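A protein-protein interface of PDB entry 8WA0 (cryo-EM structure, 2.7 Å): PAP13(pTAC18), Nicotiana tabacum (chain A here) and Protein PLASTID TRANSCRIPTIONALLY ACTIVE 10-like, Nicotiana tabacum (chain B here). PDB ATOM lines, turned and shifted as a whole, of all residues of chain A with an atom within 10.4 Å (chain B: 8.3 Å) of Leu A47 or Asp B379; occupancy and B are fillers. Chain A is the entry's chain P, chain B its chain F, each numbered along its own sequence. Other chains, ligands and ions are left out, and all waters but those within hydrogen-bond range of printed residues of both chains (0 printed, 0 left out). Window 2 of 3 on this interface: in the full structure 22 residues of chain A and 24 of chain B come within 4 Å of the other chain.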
ATOM      1  N   GLU A  41     -10.865 -12.387 -17.230  1.00  0.00           N
ATOM      2  CA  GLU A  41     -12.050 -13.220 -17.246  1.00  0.00           C
ATOM      3  C   GLU A  41     -13.212 -12.436 -17.782  1.00  0.00           C
ATOM      4  O   GLU A  41     -13.713 -12.726 -18.866  1.00  0.00           O
ATOM      5  CB  GLU A  41     -12.370 -13.715 -15.845  1.00  0.00           C
ATOM      6  N   LYS A  42     -13.654 -11.442 -17.033  1.00  0.00           N
ATOM      7  CA  LYS A  42     -14.714 -10.593 -17.495  1.00  0.00           C
ATOM      8  C   LYS A  42     -14.165  -9.910 -18.693  1.00  0.00           C
ATOM      9  O   LYS A  42     -13.006  -9.515 -18.696  1.00  0.00           O
ATOM     10  CB  LYS A  42     -14.986  -9.540 -16.437  1.00  0.00           C
ATOM     11  N   PRO A  43     -15.007  -9.674 -19.732  1.00  0.00           N
ATOM     12  CA  PRO A  43     -14.402  -8.902 -20.819  1.00  0.00           C
ATOM     13  C   PRO A  43     -14.009  -7.521 -20.332  1.00  0.00           C
ATOM     14  O   PRO A  43     -14.621  -6.988 -19.408  1.00  0.00           O
ATOM     15  CB  PRO A  43     -15.524  -8.795 -21.850  1.00  0.00           C
ATOM     16  CG  PRO A  43     -16.779  -9.035 -21.091  1.00  0.00           C
ATOM     17  CD  PRO A  43     -16.391 -10.067 -20.083  1.00  0.00           C
ATOM     18  N   LEU A  44     -13.036  -6.908 -20.981  1.00  0.00           N
ATOM     19  CA  LEU A  44     -12.549  -5.614 -20.535  1.00  0.00           C
ATOM     20  C   LEU A  44     -13.657  -4.608 -20.574  1.00  0.00           C
ATOM     21  O   LEU A  44     -13.695  -3.694 -19.761  1.00  0.00           O
ATOM     22  CB  LEU A  44     -11.416  -5.137 -21.434  1.00  0.00           C
ATOM     23  CG  LEU A  44      -9.978  -5.349 -20.973  1.00  0.00           C
ATOM     24  CD1 LEU A  44      -9.023  -4.789 -22.014  1.00  0.00           C
ATOM     25  CD2 LEU A  44      -9.754  -4.673 -19.631  1.00  0.00           C
ATOM     26  N   GLU A  45     -14.562  -4.756 -21.523  1.00  0.00           N
ATOM     27  CA  GLU A  45     -15.600  -3.762 -21.690  1.00  0.00           C
ATOM     28  C   GLU A  45     -16.447  -3.616 -20.456  1.00  0.00           C
ATOM     29  O   GLU A  45     -16.763  -2.505 -20.058  1.00  0.00           O
ATOM     30  CB  GLU A  45     -16.510  -4.167 -22.843  1.00  0.00           C
ATOM     31  N   GLU A  46     -16.820  -4.722 -19.839  1.00  0.00           N
ATOM     32  CA  GLU A  46     -17.703  -4.620 -18.697  1.00  0.00           C
ATOM     33  C   GLU A  46     -16.997  -3.867 -17.591  1.00  0.00           C
ATOM     34  O   GLU A  46     -17.597  -3.044 -16.913  1.00  0.00           O
ATOM     35  CB  GLU A  46     -18.214  -5.999 -18.259  1.00  0.00           C
ATOM     36  N   LEU A  47     -15.715  -4.140 -17.416  1.00  0.00           N
ATOM     37  CA  LEU A  47     -14.958  -3.494 -16.369  1.00  0.00           C
ATOM     38  C   LEU A  47     -14.899  -2.008 -16.618  1.00  0.00           C
ATOM     39  O   LEU A  47     -15.032  -1.211 -15.694  1.00  0.00           O
ATOM     40  CB  LEU A  47     -13.546  -4.069 -16.350  1.00  0.00           C
ATOM     41  CG  LEU A  47     -12.691  -3.868 -15.106  1.00  0.00           C
ATOM     42  CD1 LEU A  47     -13.284  -4.650 -13.947  1.00  0.00           C
ATOM     43  CD2 LEU A  47     -11.267  -4.319 -15.377  1.00  0.00           C
ATOM     44  N   TYR A  48     -14.711  -1.620 -17.868  1.00  0.00           N
ATOM     45  CA  TYR A  48     -14.559  -0.211 -18.174  1.00  0.00           C
ATOM     46  C   TYR A  48     -15.864   0.474 -18.527  1.00  0.00           C
ATOM     47  O   TYR A  48     -15.874   1.666 -18.807  1.00  0.00           O
ATOM     48  CB  TYR A  48     -13.532  -0.043 -19.279  1.00  0.00           C
ATOM     49  CG  TYR A  48     -12.107  -0.026 -18.786  1.00  0.00           C
ATOM     50  CD1 TYR A  48     -11.392  -1.201 -18.615  1.00  0.00           C
ATOM     51  CD2 TYR A  48     -11.478   1.170 -18.492  1.00  0.00           C
ATOM     52  CE1 TYR A  48     -10.088  -1.180 -18.163  1.00  0.00           C
ATOM     53  CE2 TYR A  48     -10.176   1.203 -18.044  1.00  0.00           C
ATOM     54  CZ  TYR A  48      -9.487   0.027 -17.878  1.00  0.00           C
ATOM     55  OH  TYR A  48      -8.190   0.068 -17.430  1.00  0.00           O
ATOM     56  N   ASN A  49     -16.964  -0.266 -18.501  1.00  0.00           N
ATOM     57  CA  ASN A  49     -18.291   0.287 -18.823  1.00  0.00           C
ATOM     58  C   ASN A  49     -18.501   0.897 -20.186  1.00  0.00           C
ATOM     59  O   ASN A  49     -19.156   1.926 -20.308  1.00  0.00           O
ATOM     60  CB  ASN A  49     -18.818   1.218 -17.733  1.00  0.00           C
ATOM     61  CG  ASN A  49     -19.859   0.548 -16.866  1.00  0.00           C
ATOM     62  OD1 ASN A  49     -20.679  -0.228 -17.355  1.00  0.00           O
ATOM     63  ND2 ASN A  49     -19.832   0.842 -15.573  1.00  0.00           N
ATOM     64  N   VAL A  50     -17.947   0.279 -21.216  1.00  0.00           N
ATOM     65  CA  VAL A  50     -18.240   0.741 -22.556  1.00  0.00           C
ATOM     66  C   VAL A  50     -19.321  -0.224 -22.982  1.00  0.00           C
ATOM     67  O   VAL A  50     -19.051  -1.396 -23.217  1.00  0.00           O
ATOM     68  CB  VAL A  50     -17.040   0.566 -23.480  1.00  0.00           C
ATOM     69  N   ARG A  51     -20.549   0.254 -23.081  1.00  0.00           N
ATOM     70  CA  ARG A  51     -21.646  -0.624 -23.422  1.00  0.00           C
ATOM     71  C   ARG A  51     -21.760  -0.631 -24.927  1.00  0.00           C
ATOM     72  O   ARG A  51     -21.693   0.428 -25.549  1.00  0.00           O
ATOM     73  CB  ARG A  51     -22.931  -0.093 -22.812  1.00  0.00           C
ATOM     74  CG  ARG A  51     -22.727   0.652 -21.506  1.00  0.00           C
ATOM     75  CD  ARG A  51     -23.906   1.562 -21.220  1.00  0.00           C
ATOM     76  NE  ARG A  51     -23.566   2.595 -20.249  1.00  0.00           N
ATOM     77  CZ  ARG A  51     -24.351   3.623 -19.948  1.00  0.00           C
ATOM     78  NH1 ARG A  51     -25.525   3.761 -20.547  1.00  0.00           N
ATOM     79  NH2 ARG A  51     -23.960   4.517 -19.053  1.00  0.00           N
ATOM     80  N   PRO A 100      -7.021   0.557 -23.269  1.00  0.00           N
ATOM     81  CA  PRO A 100      -7.155   1.441 -22.123  1.00  0.00           C
ATOM     82  C   PRO A 100      -5.784   1.753 -21.582  1.00  0.00           C
ATOM     83  O   PRO A 100      -4.918   0.898 -21.602  1.00  0.00           O
ATOM     84  CB  PRO A 100      -7.938   0.601 -21.132  1.00  0.00           C
ATOM     85  CG  PRO A 100      -8.713  -0.352 -21.970  1.00  0.00           C
ATOM     86  CD  PRO A 100      -7.815  -0.674 -23.122  1.00  0.00           C
ATOM     87  N   GLU A 101      -5.574   2.973 -21.124  1.00  0.00           N
ATOM     88  CA  GLU A 101      -4.256   3.377 -20.648  1.00  0.00           C
ATOM     89  C   GLU A 101      -3.530   2.354 -19.786  1.00  0.00           C
ATOM     90  O   GLU A 101      -4.007   1.997 -18.712  1.00  0.00           O
ATOM     91  CB  GLU A 101      -4.367   4.710 -19.902  1.00  0.00           C
ATOM     92  CG  GLU A 101      -3.100   5.170 -19.197  1.00  0.00           C
ATOM     93  CD  GLU A 101      -2.062   5.743 -20.140  1.00  0.00           C
ATOM     94  OE1 GLU A 101      -2.271   5.701 -21.368  1.00  0.00           O
ATOM     95  OE2 GLU A 101      -1.028   6.243 -19.650  1.00  0.00           O
ATOM     96  N   SER A 103      -2.853  -0.716 -20.536  1.00  0.00           N
ATOM     97  CA  SER A 103      -3.199  -2.075 -20.758  1.00  0.00           C
ATOM     98  C   SER A 103      -2.280  -2.768 -21.663  1.00  0.00           C
ATOM     99  O   SER A 103      -1.599  -2.154 -22.464  1.00  0.00           O
ATOM    100  CB  SER A 103      -4.596  -2.207 -21.303  1.00  0.00           C
ATOM    101  OG  SER A 103      -4.643  -1.750 -22.640  1.00  0.00           O
ATOM    102  N   ARG A 105      -3.775  -5.273 -22.979  1.00  0.00           N
ATOM    103  CA  ARG A 105      -4.870  -5.963 -23.659  1.00  0.00           C
ATOM    104  C   ARG A 105      -5.803  -4.985 -24.363  1.00  0.00           C
ATOM    105  O   ARG A 105      -5.894  -3.833 -23.955  1.00  0.00           O
ATOM    106  CB  ARG A 105      -5.638  -6.840 -22.688  1.00  0.00           C
ATOM    107  CG  ARG A 105      -4.907  -8.116 -22.311  1.00  0.00           C
ATOM    108  CD  ARG A 105      -5.652  -8.915 -21.254  1.00  0.00           C
ATOM    109  NE  ARG A 105      -5.860  -8.152 -20.027  1.00  0.00           N
ATOM    110  CZ  ARG A 105      -7.054  -7.839 -19.535  1.00  0.00           C
ATOM    111  NH1 ARG A 105      -8.154  -8.236 -20.160  1.00  0.00           N
ATOM    112  NH2 ARG A 105      -7.148  -7.140 -18.413  1.00  0.00           N
ATOM    113  N   MET A 107      -9.526  -3.820 -26.884  1.00  0.00           N
ATOM    114  CA  MET A 107     -10.907  -4.066 -27.241  1.00  0.00           C
ATOM    115  C   MET A 107     -10.998  -3.794 -28.730  1.00  0.00           C
ATOM    116  O   MET A 107     -10.630  -2.710 -29.175  1.00  0.00           O
ATOM    117  CB  MET A 107     -11.802  -3.070 -26.532  1.00  0.00           C
ATOM    118  CG  MET A 107     -11.527  -2.880 -25.051  1.00  0.00           C
ATOM    119  SD  MET A 107     -12.512  -1.519 -24.393  1.00  0.00           S
ATOM    120  CE  MET A 107     -12.170  -1.657 -22.642  1.00  0.00           C
ATOM    121  N   PRO A 118     -17.530   6.023 -22.075  1.00  0.00           N
ATOM    122  CA  PRO A 118     -17.922   6.723 -20.846  1.00  0.00           C
ATOM    123  C   PRO A 118     -17.335   8.083 -20.543  1.00  0.00           C
ATOM    124  O   PRO A 118     -16.267   8.395 -21.016  1.00  0.00           O
ATOM    125  CB  PRO A 118     -17.527   5.748 -19.763  1.00  0.00           C
ATOM    126  CG  PRO A 118     -16.404   4.959 -20.334  1.00  0.00           C
ATOM    127  CD  PRO A 118     -16.575   4.935 -21.823  1.00  0.00           C
ATOM    128  N   PHE A 121     -13.619   8.771 -19.403  1.00  0.00           N
ATOM    129  CA  PHE A 121     -12.810   7.693 -19.971  1.00  0.00           C
ATOM    130  C   PHE A 121     -11.584   8.216 -20.669  1.00  0.00           C
ATOM    131  O   PHE A 121     -11.653   9.212 -21.364  1.00  0.00           O
ATOM    132  CB  PHE A 121     -13.611   6.884 -20.969  1.00  0.00           C
ATOM    133  CG  PHE A 121     -12.940   5.623 -21.422  1.00  0.00           C
ATOM    134  CD1 PHE A 121     -12.296   4.799 -20.520  1.00  0.00           C
ATOM    135  CD2 PHE A 121     -12.992   5.240 -22.747  1.00  0.00           C
ATOM    136  CE1 PHE A 121     -11.688   3.633 -20.941  1.00  0.00           C
ATOM    137  CE2 PHE A 121     -12.393   4.075 -23.174  1.00  0.00           C
ATOM    138  CZ  PHE A 121     -11.740   3.268 -22.268  1.00  0.00           C
ATOM    139  N   ARG B 333     -18.011 -12.932  -2.277  1.00  0.00           N
ATOM    140  CA  ARG B 333     -17.108 -12.349  -3.212  1.00  0.00           C
ATOM    141  C   ARG B 333     -16.270 -13.412  -3.918  1.00  0.00           C
ATOM    142  O   ARG B 333     -16.253 -14.550  -3.490  1.00  0.00           O
ATOM    143  CB  ARG B 333     -16.241 -11.348  -2.500  1.00  0.00           C
ATOM    144  CG  ARG B 333     -16.934 -10.157  -1.882  1.00  0.00           C
ATOM    145  CD  ARG B 333     -15.922  -9.302  -1.152  1.00  0.00           C
ATOM    146  NE  ARG B 333     -16.527  -8.443  -0.150  1.00  0.00           N
ATOM    147  CZ  ARG B 333     -16.880  -7.185  -0.364  1.00  0.00           C
ATOM    148  NH1 ARG B 333     -16.689  -6.634  -1.548  1.00  0.00           N
ATOM    149  NH2 ARG B 333     -17.423  -6.478   0.613  1.00  0.00           N
ATOM    150  N   ASP B 334     -15.600 -13.063  -5.007  1.00  0.00           N
ATOM    151  CA  ASP B 334     -14.760 -13.990  -5.777  1.00  0.00           C
ATOM    152  C   ASP B 334     -13.533 -14.517  -5.091  1.00  0.00           C
ATOM    153  O   ASP B 334     -12.819 -13.782  -4.440  1.00  0.00           O
ATOM    154  CB  ASP B 334     -14.281 -13.239  -6.998  1.00  0.00           C
ATOM    155  CG  ASP B 334     -13.464 -14.094  -7.938  1.00  0.00           C
ATOM    156  OD1 ASP B 334     -13.963 -15.147  -8.385  1.00  0.00           O
ATOM    157  OD2 ASP B 334     -12.317 -13.704  -8.240  1.00  0.00           O
ATOM    158  N   TYR B 336     -10.556 -15.532  -6.461  1.00  0.00           N
ATOM    159  CA  TYR B 336      -9.291 -15.078  -6.975  1.00  0.00           C
ATOM    160  C   TYR B 336      -8.838 -13.691  -6.515  1.00  0.00           C
ATOM    161  O   TYR B 336      -7.683 -13.535  -6.169  1.00  0.00           O
ATOM    162  CB  TYR B 336      -9.293 -15.210  -8.490  1.00  0.00           C
ATOM    163  CG  TYR B 336      -8.009 -14.857  -9.207  1.00  0.00           C
ATOM    164  CD1 TYR B 336      -7.664 -13.541  -9.454  1.00  0.00           C
ATOM    165  CD2 TYR B 336      -7.158 -15.844  -9.656  1.00  0.00           C
ATOM    166  CE1 TYR B 336      -6.495 -13.220 -10.098  1.00  0.00           C
ATOM    167  CE2 TYR B 336      -5.989 -15.532 -10.306  1.00  0.00           C
ATOM    168  CZ  TYR B 336      -5.666 -14.222 -10.529  1.00  0.00           C
ATOM    169  OH  TYR B 336      -4.497 -13.908 -11.183  1.00  0.00           O
ATOM    170  N   ARG B 337      -9.690 -12.691  -6.497  1.00  0.00           N
ATOM    171  CA  ARG B 337      -9.283 -11.378  -6.066  1.00  0.00           C
ATOM    172  C   ARG B 337      -9.398 -11.143  -4.608  1.00  0.00           C
ATOM    173  O   ARG B 337      -8.608 -10.409  -4.039  1.00  0.00           O
ATOM    174  CB  ARG B 337      -9.919 -10.236  -6.849  1.00  0.00           C
ATOM    175  CG  ARG B 337      -9.241  -8.893  -6.741  1.00  0.00           C
ATOM    176  CD  ARG B 337      -7.781  -8.981  -7.124  1.00  0.00           C
ATOM    177  NE  ARG B 337      -7.576  -8.800  -8.547  1.00  0.00           N
ATOM    178  CZ  ARG B 337      -6.408  -8.964  -9.153  1.00  0.00           C
ATOM    179  NH1 ARG B 337      -5.343  -9.324  -8.451  1.00  0.00           N
ATOM    180  NH2 ARG B 337      -6.305  -8.778 -10.459  1.00  0.00           N
ATOM    181  N   PHE B 338     -10.323 -11.786  -3.950  1.00  0.00           N
ATOM    182  CA  PHE B 338     -10.533 -11.488  -2.567  1.00  0.00           C
ATOM    183  C   PHE B 338     -10.084 -12.595  -1.657  1.00  0.00           C
ATOM    184  O   PHE B 338     -10.443 -13.732  -1.860  1.00  0.00           O
ATOM    185  CB  PHE B 338     -11.983 -11.132  -2.367  1.00  0.00           C
ATOM    186  CG  PHE B 338     -12.354  -9.777  -2.853  1.00  0.00           C
ATOM    187  CD1 PHE B 338     -12.112  -8.674  -2.076  1.00  0.00           C
ATOM    188  CD2 PHE B 338     -12.969  -9.615  -4.067  1.00  0.00           C
ATOM    189  CE1 PHE B 338     -12.455  -7.422  -2.509  1.00  0.00           C
ATOM    190  CE2 PHE B 338     -13.315  -8.367  -4.513  1.00  0.00           C
ATOM    191  CZ  PHE B 338     -13.061  -7.266  -3.731  1.00  0.00           C
ATOM    192  N   ILE B 364      -7.392  -7.954  -0.457  1.00  0.00           N
ATOM    193  CA  ILE B 364      -7.305  -8.556  -1.792  1.00  0.00           C
ATOM    194  C   ILE B 364      -5.951  -9.192  -2.065  1.00  0.00           C
ATOM    195  O   ILE B 364      -5.034  -9.019  -1.280  1.00  0.00           O
ATOM    196  CB  ILE B 364      -7.497  -7.499  -2.881  1.00  0.00           C
ATOM    197  CG1 ILE B 364      -6.454  -6.395  -2.732  1.00  0.00           C
ATOM    198  CG2 ILE B 364      -8.890  -6.909  -2.825  1.00  0.00           C
ATOM    199  CD1 ILE B 364      -6.337  -5.504  -3.944  1.00  0.00           C
ATOM    200  N   ASN B 372      -1.753  -3.427 -14.631  1.00  0.00           N
ATOM    201  CA  ASN B 372      -2.388  -2.137 -14.600  1.00  0.00           C
ATOM    202  C   ASN B 372      -3.043  -1.930 -13.270  1.00  0.00           C
ATOM    203  O   ASN B 372      -3.943  -2.668 -12.891  1.00  0.00           O
ATOM    204  CB  ASN B 372      -3.420  -2.025 -15.708  1.00  0.00           C
ATOM    205  CG  ASN B 372      -3.830  -0.592 -15.981  1.00  0.00           C
ATOM    206  OD1 ASN B 372      -3.383   0.336 -15.308  1.00  0.00           O
ATOM    207  ND2 ASN B 372      -4.679  -0.404 -16.981  1.00  0.00           N
ATOM    208  N   LEU B 373      -2.593  -0.914 -12.555  1.00  0.00           N
ATOM    209  CA  LEU B 373      -3.182  -0.594 -11.278  1.00  0.00           C
ATOM    210  C   LEU B 373      -4.613  -0.161 -11.482  1.00  0.00           C
ATOM    211  O   LEU B 373      -5.481  -0.470 -10.673  1.00  0.00           O
ATOM    212  CB  LEU B 373      -2.380   0.501 -10.609  1.00  0.00           C
ATOM    213  CG  LEU B 373      -0.873   0.255 -10.612  1.00  0.00           C
ATOM    214  CD1 LEU B 373      -0.142   1.401  -9.933  1.00  0.00           C
ATOM    215  CD2 LEU B 373      -0.522  -1.069  -9.950  1.00  0.00           C
ATOM    216  N   ASP B 374      -4.865   0.573 -12.555  1.00  0.00           N
ATOM    217  CA  ASP B 374      -6.208   1.066 -12.829  1.00  0.00           C
ATOM    218  C   ASP B 374      -7.209  -0.048 -13.061  1.00  0.00           C
ATOM    219  O   ASP B 374      -8.343   0.023 -12.593  1.00  0.00           O
ATOM    220  CB  ASP B 374      -6.179   1.992 -14.033  1.00  0.00           C
ATOM    221  CG  ASP B 374      -7.391   2.884 -14.106  1.00  0.00           C
ATOM    222  OD1 ASP B 374      -7.941   3.228 -13.038  1.00  0.00           O
ATOM    223  OD2 ASP B 374      -7.790   3.250 -15.231  1.00  0.00           O
ATOM    224  N   GLU B 375      -6.804  -1.085 -13.772  1.00  0.00           N
ATOM    225  CA  GLU B 375      -7.690  -2.209 -13.971  1.00  0.00           C
ATOM    226  C   GLU B 375      -8.005  -2.840 -12.637  1.00  0.00           C
ATOM    227  O   GLU B 375      -9.141  -3.216 -12.373  1.00  0.00           O
ATOM    228  CB  GLU B 375      -7.029  -3.242 -14.864  1.00  0.00           C
ATOM    229  CG  GLU B 375      -6.983  -2.873 -16.333  1.00  0.00           C
ATOM    230  CD  GLU B 375      -6.166  -3.853 -17.150  1.00  0.00           C
ATOM    231  OE1 GLU B 375      -5.776  -4.903 -16.601  1.00  0.00           O
ATOM    232  OE2 GLU B 375      -5.908  -3.573 -18.338  1.00  0.00           O
ATOM    233  N   LEU B 376      -7.003  -2.948 -11.784  1.00  0.00           N
ATOM    234  CA  LEU B 376      -7.196  -3.558 -10.482  1.00  0.00           C
ATOM    235  C   LEU B 376      -8.181  -2.784  -9.636  1.00  0.00           C
ATOM    236  O   LEU B 376      -9.031  -3.377  -8.987  1.00  0.00           O
ATOM    237  CB  LEU B 376      -5.852  -3.647  -9.766  1.00  0.00           C
ATOM    238  CG  LEU B 376      -5.741  -4.159  -8.334  1.00  0.00           C
ATOM    239  CD1 LEU B 376      -6.068  -5.636  -8.291  1.00  0.00           C
ATOM    240  CD2 LEU B 376      -4.332  -3.929  -7.817  1.00  0.00           C
ATOM    241  N   ARG B 377      -8.119  -1.462  -9.677  1.00  0.00           N
ATOM    242  CA  ARG B 377      -8.972  -0.679  -8.805  1.00  0.00           C
ATOM    243  C   ARG B 377     -10.403  -0.995  -9.108  1.00  0.00           C
ATOM    244  O   ARG B 377     -11.227  -1.087  -8.208  1.00  0.00           O
ATOM    245  CB  ARG B 377      -8.741   0.808  -9.016  1.00  0.00           C
ATOM    246  N   ARG B 378     -10.711  -1.148 -10.383  1.00  0.00           N
ATOM    247  CA  ARG B 378     -12.074  -1.439 -10.774  1.00  0.00           C
ATOM    248  C   ARG B 378     -12.621  -2.775 -10.283  1.00  0.00           C
ATOM    249  O   ARG B 378     -13.765  -2.844  -9.846  1.00  0.00           O
ATOM    250  CB  ARG B 378     -12.209  -1.344 -12.281  1.00  0.00           C
ATOM    251  CG  ARG B 378     -12.222   0.075 -12.813  1.00  0.00           C
ATOM    252  CD  ARG B 378     -12.009   0.093 -14.318  1.00  0.00           C
ATOM    253  NE  ARG B 378     -12.551   1.302 -14.929  1.00  0.00           N
ATOM    254  CZ  ARG B 378     -11.883   2.442 -15.055  1.00  0.00           C
ATOM    255  NH1 ARG B 378     -10.640   2.536 -14.612  1.00  0.00           N
ATOM    256  NH2 ARG B 378     -12.457   3.488 -15.627  1.00  0.00           N
ATOM    257  N   ASP B 379     -11.826  -3.834 -10.343  1.00  0.00           N
ATOM    258  CA  ASP B 379     -12.317  -5.152  -9.949  1.00  0.00           C
ATOM    259  C   ASP B 379     -12.587  -5.180  -8.457  1.00  0.00           C
ATOM    260  O   ASP B 379     -13.595  -5.720  -8.023  1.00  0.00           O
ATOM    261  CB  ASP B 379     -11.293  -6.205 -10.335  1.00  0.00           C
ATOM    262  CG  ASP B 379     -11.886  -7.593 -10.431  1.00  0.00           C
ATOM    263  OD1 ASP B 379     -13.106  -7.744 -10.218  1.00  0.00           O
ATOM    264  OD2 ASP B 379     -11.127  -8.537 -10.731  1.00  0.00           O
ATOM    265  N   CYS B 380     -11.693  -4.618  -7.664  1.00  0.00           N
ATOM    266  CA  CYS B 380     -11.850  -4.521  -6.237  1.00  0.00           C
ATOM    267  C   CYS B 380     -12.901  -3.621  -5.668  1.00  0.00           C
ATOM    268  O   CYS B 380     -13.600  -3.998  -4.753  1.00  0.00           O
ATOM    269  CB  CYS B 380     -10.527  -4.113  -5.674  1.00  0.00           C
ATOM    270  SG  CYS B 380      -9.165  -5.124  -6.277  1.00  0.00           S
ATOM    271  N   GLY B 381     -13.067  -2.436  -6.208  1.00  0.00           N
ATOM    272  CA  GLY B 381     -13.979  -1.502  -5.600  1.00  0.00           C
ATOM    273  C   GLY B 381     -13.341  -0.328  -4.936  1.00  0.00           C
ATOM    274  O   GLY B 381     -13.952   0.289  -4.092  1.00  0.00           O
ATOM    275  N   ARG B 382     -12.104  -0.093  -5.253  1.00  0.00           N
ATOM    276  CA  ARG B 382     -11.407   0.901  -4.544  1.00  0.00           C
ATOM    277  C   ARG B 382     -11.351   2.179  -5.276  1.00  0.00           C
ATOM    278  O   ARG B 382     -11.572   2.210  -6.473  1.00  0.00           O
ATOM    279  CB  ARG B 382     -10.039   0.337  -4.213  1.00  0.00           C
ATOM    280  CG  ARG B 382     -10.117  -0.891  -3.323  1.00  0.00           C
ATOM    281  CD  ARG B 382      -8.757  -1.447  -2.962  1.00  0.00           C
ATOM    282  NE  ARG B 382      -8.859  -2.451  -1.910  1.00  0.00           N
ATOM    283  CZ  ARG B 382      -7.819  -3.045  -1.340  1.00  0.00           C
ATOM    284  NH1 ARG B 382      -6.593  -2.745  -1.717  1.00  0.00           N
ATOM    285  NH2 ARG B 382      -8.009  -3.942  -0.391  1.00  0.00           N
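The side-chain amide nitrogen (ND2) of Asn B372 sits at hydrogen-bond distance from the backbone carbonyl oxygen (O) of Glu A101 (3.0 Å).
The guanidinium group (NH2) of Arg A105 lies within salt-bridge range of the side-chain carboxylate (OE1) of Glu B375 (3.2 Å).
O of Pro A100 is in hydrogen-bond range of OG of Ser A103, 2.9 Å away.
The side-chain hydroxyl (OG) of Ser A103 lies within hydrogen-bond range of the backbone carbonyl oxygen (O) of Arg A105 (2.8 Å).
The side-chain amide oxygen (OD1) of Asn B372 lies within hydrogen-bond range of the backbone NH (N) of Asp B374, 3.1 Å away.
The side-chain carboxylate (OD2) of Asp B374 lies within salt-bridge range of the guanidinium group (NH1) of Arg B378 (3.0 Å).
Among the printed residues, pairs that only touch across the chains: Tyr A48 with Glu B375 (3.4 Å), Ser A103 with Glu B375 (3.5 Å), Leu A47 with Arg B378 (3.6 Å), Tyr A48 with Asn B372 (3.6 Å), Tyr A48 with Arg B378 (3.7 Å), Leu A47 with Glu B375 (3.8 Å), Tyr A48 with Asp B374 (3.9 Å) and Leu A47 with Asp B379 (3.97 Å).
Of chain B, only Glu B375, Arg B378 and Asp B379 come within 4 Å of Leu A47.
Printed residues of chain A within 4 Å of Asp B379: Leu A47.
Of chain A, only Leu A47 (3.8 Å), Tyr A48 (3.4 Å), Ser A103 (3.5 Å) and Arg A105 (3.2 Å) come within 4 Å of Glu B375.
Arg B378 touches just these residues of chain A: Leu A47 (3.6 Å) and Tyr A48 (3.7 Å).
No residue of chain A comes within 4 Å of Cys B380.
Of the printed residues of chain B, Tyr A48 touches Asn B372 (3.6 Å), Asp B374 (3.9 Å), Glu B375 (3.4 Å) and Arg B378 (3.7 Å).
Printed residues of chain B within 4 Å of Glu A101: Asn B372.
Ile B364 touches none of the printed residues of chain A.
The nearest residue of chain B that does not touch Leu A47 is Leu B376 (5.7 Å).
Of the 17 printed residues of chain B, 5 touch a printed residue of chain A.
Printed residues of chain A that touch a printed residue of chain B: Leu A47, Tyr A48, Glu A101, Ser A103 and Arg A105.
Among the printed residues, 10 pairs touch across the chains.
Among the printed residues, Asp or Glu carboxylates within 4 Å of a Lys or Arg side-chain nitrogen of the other chain: Arg A105 with Glu B375.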
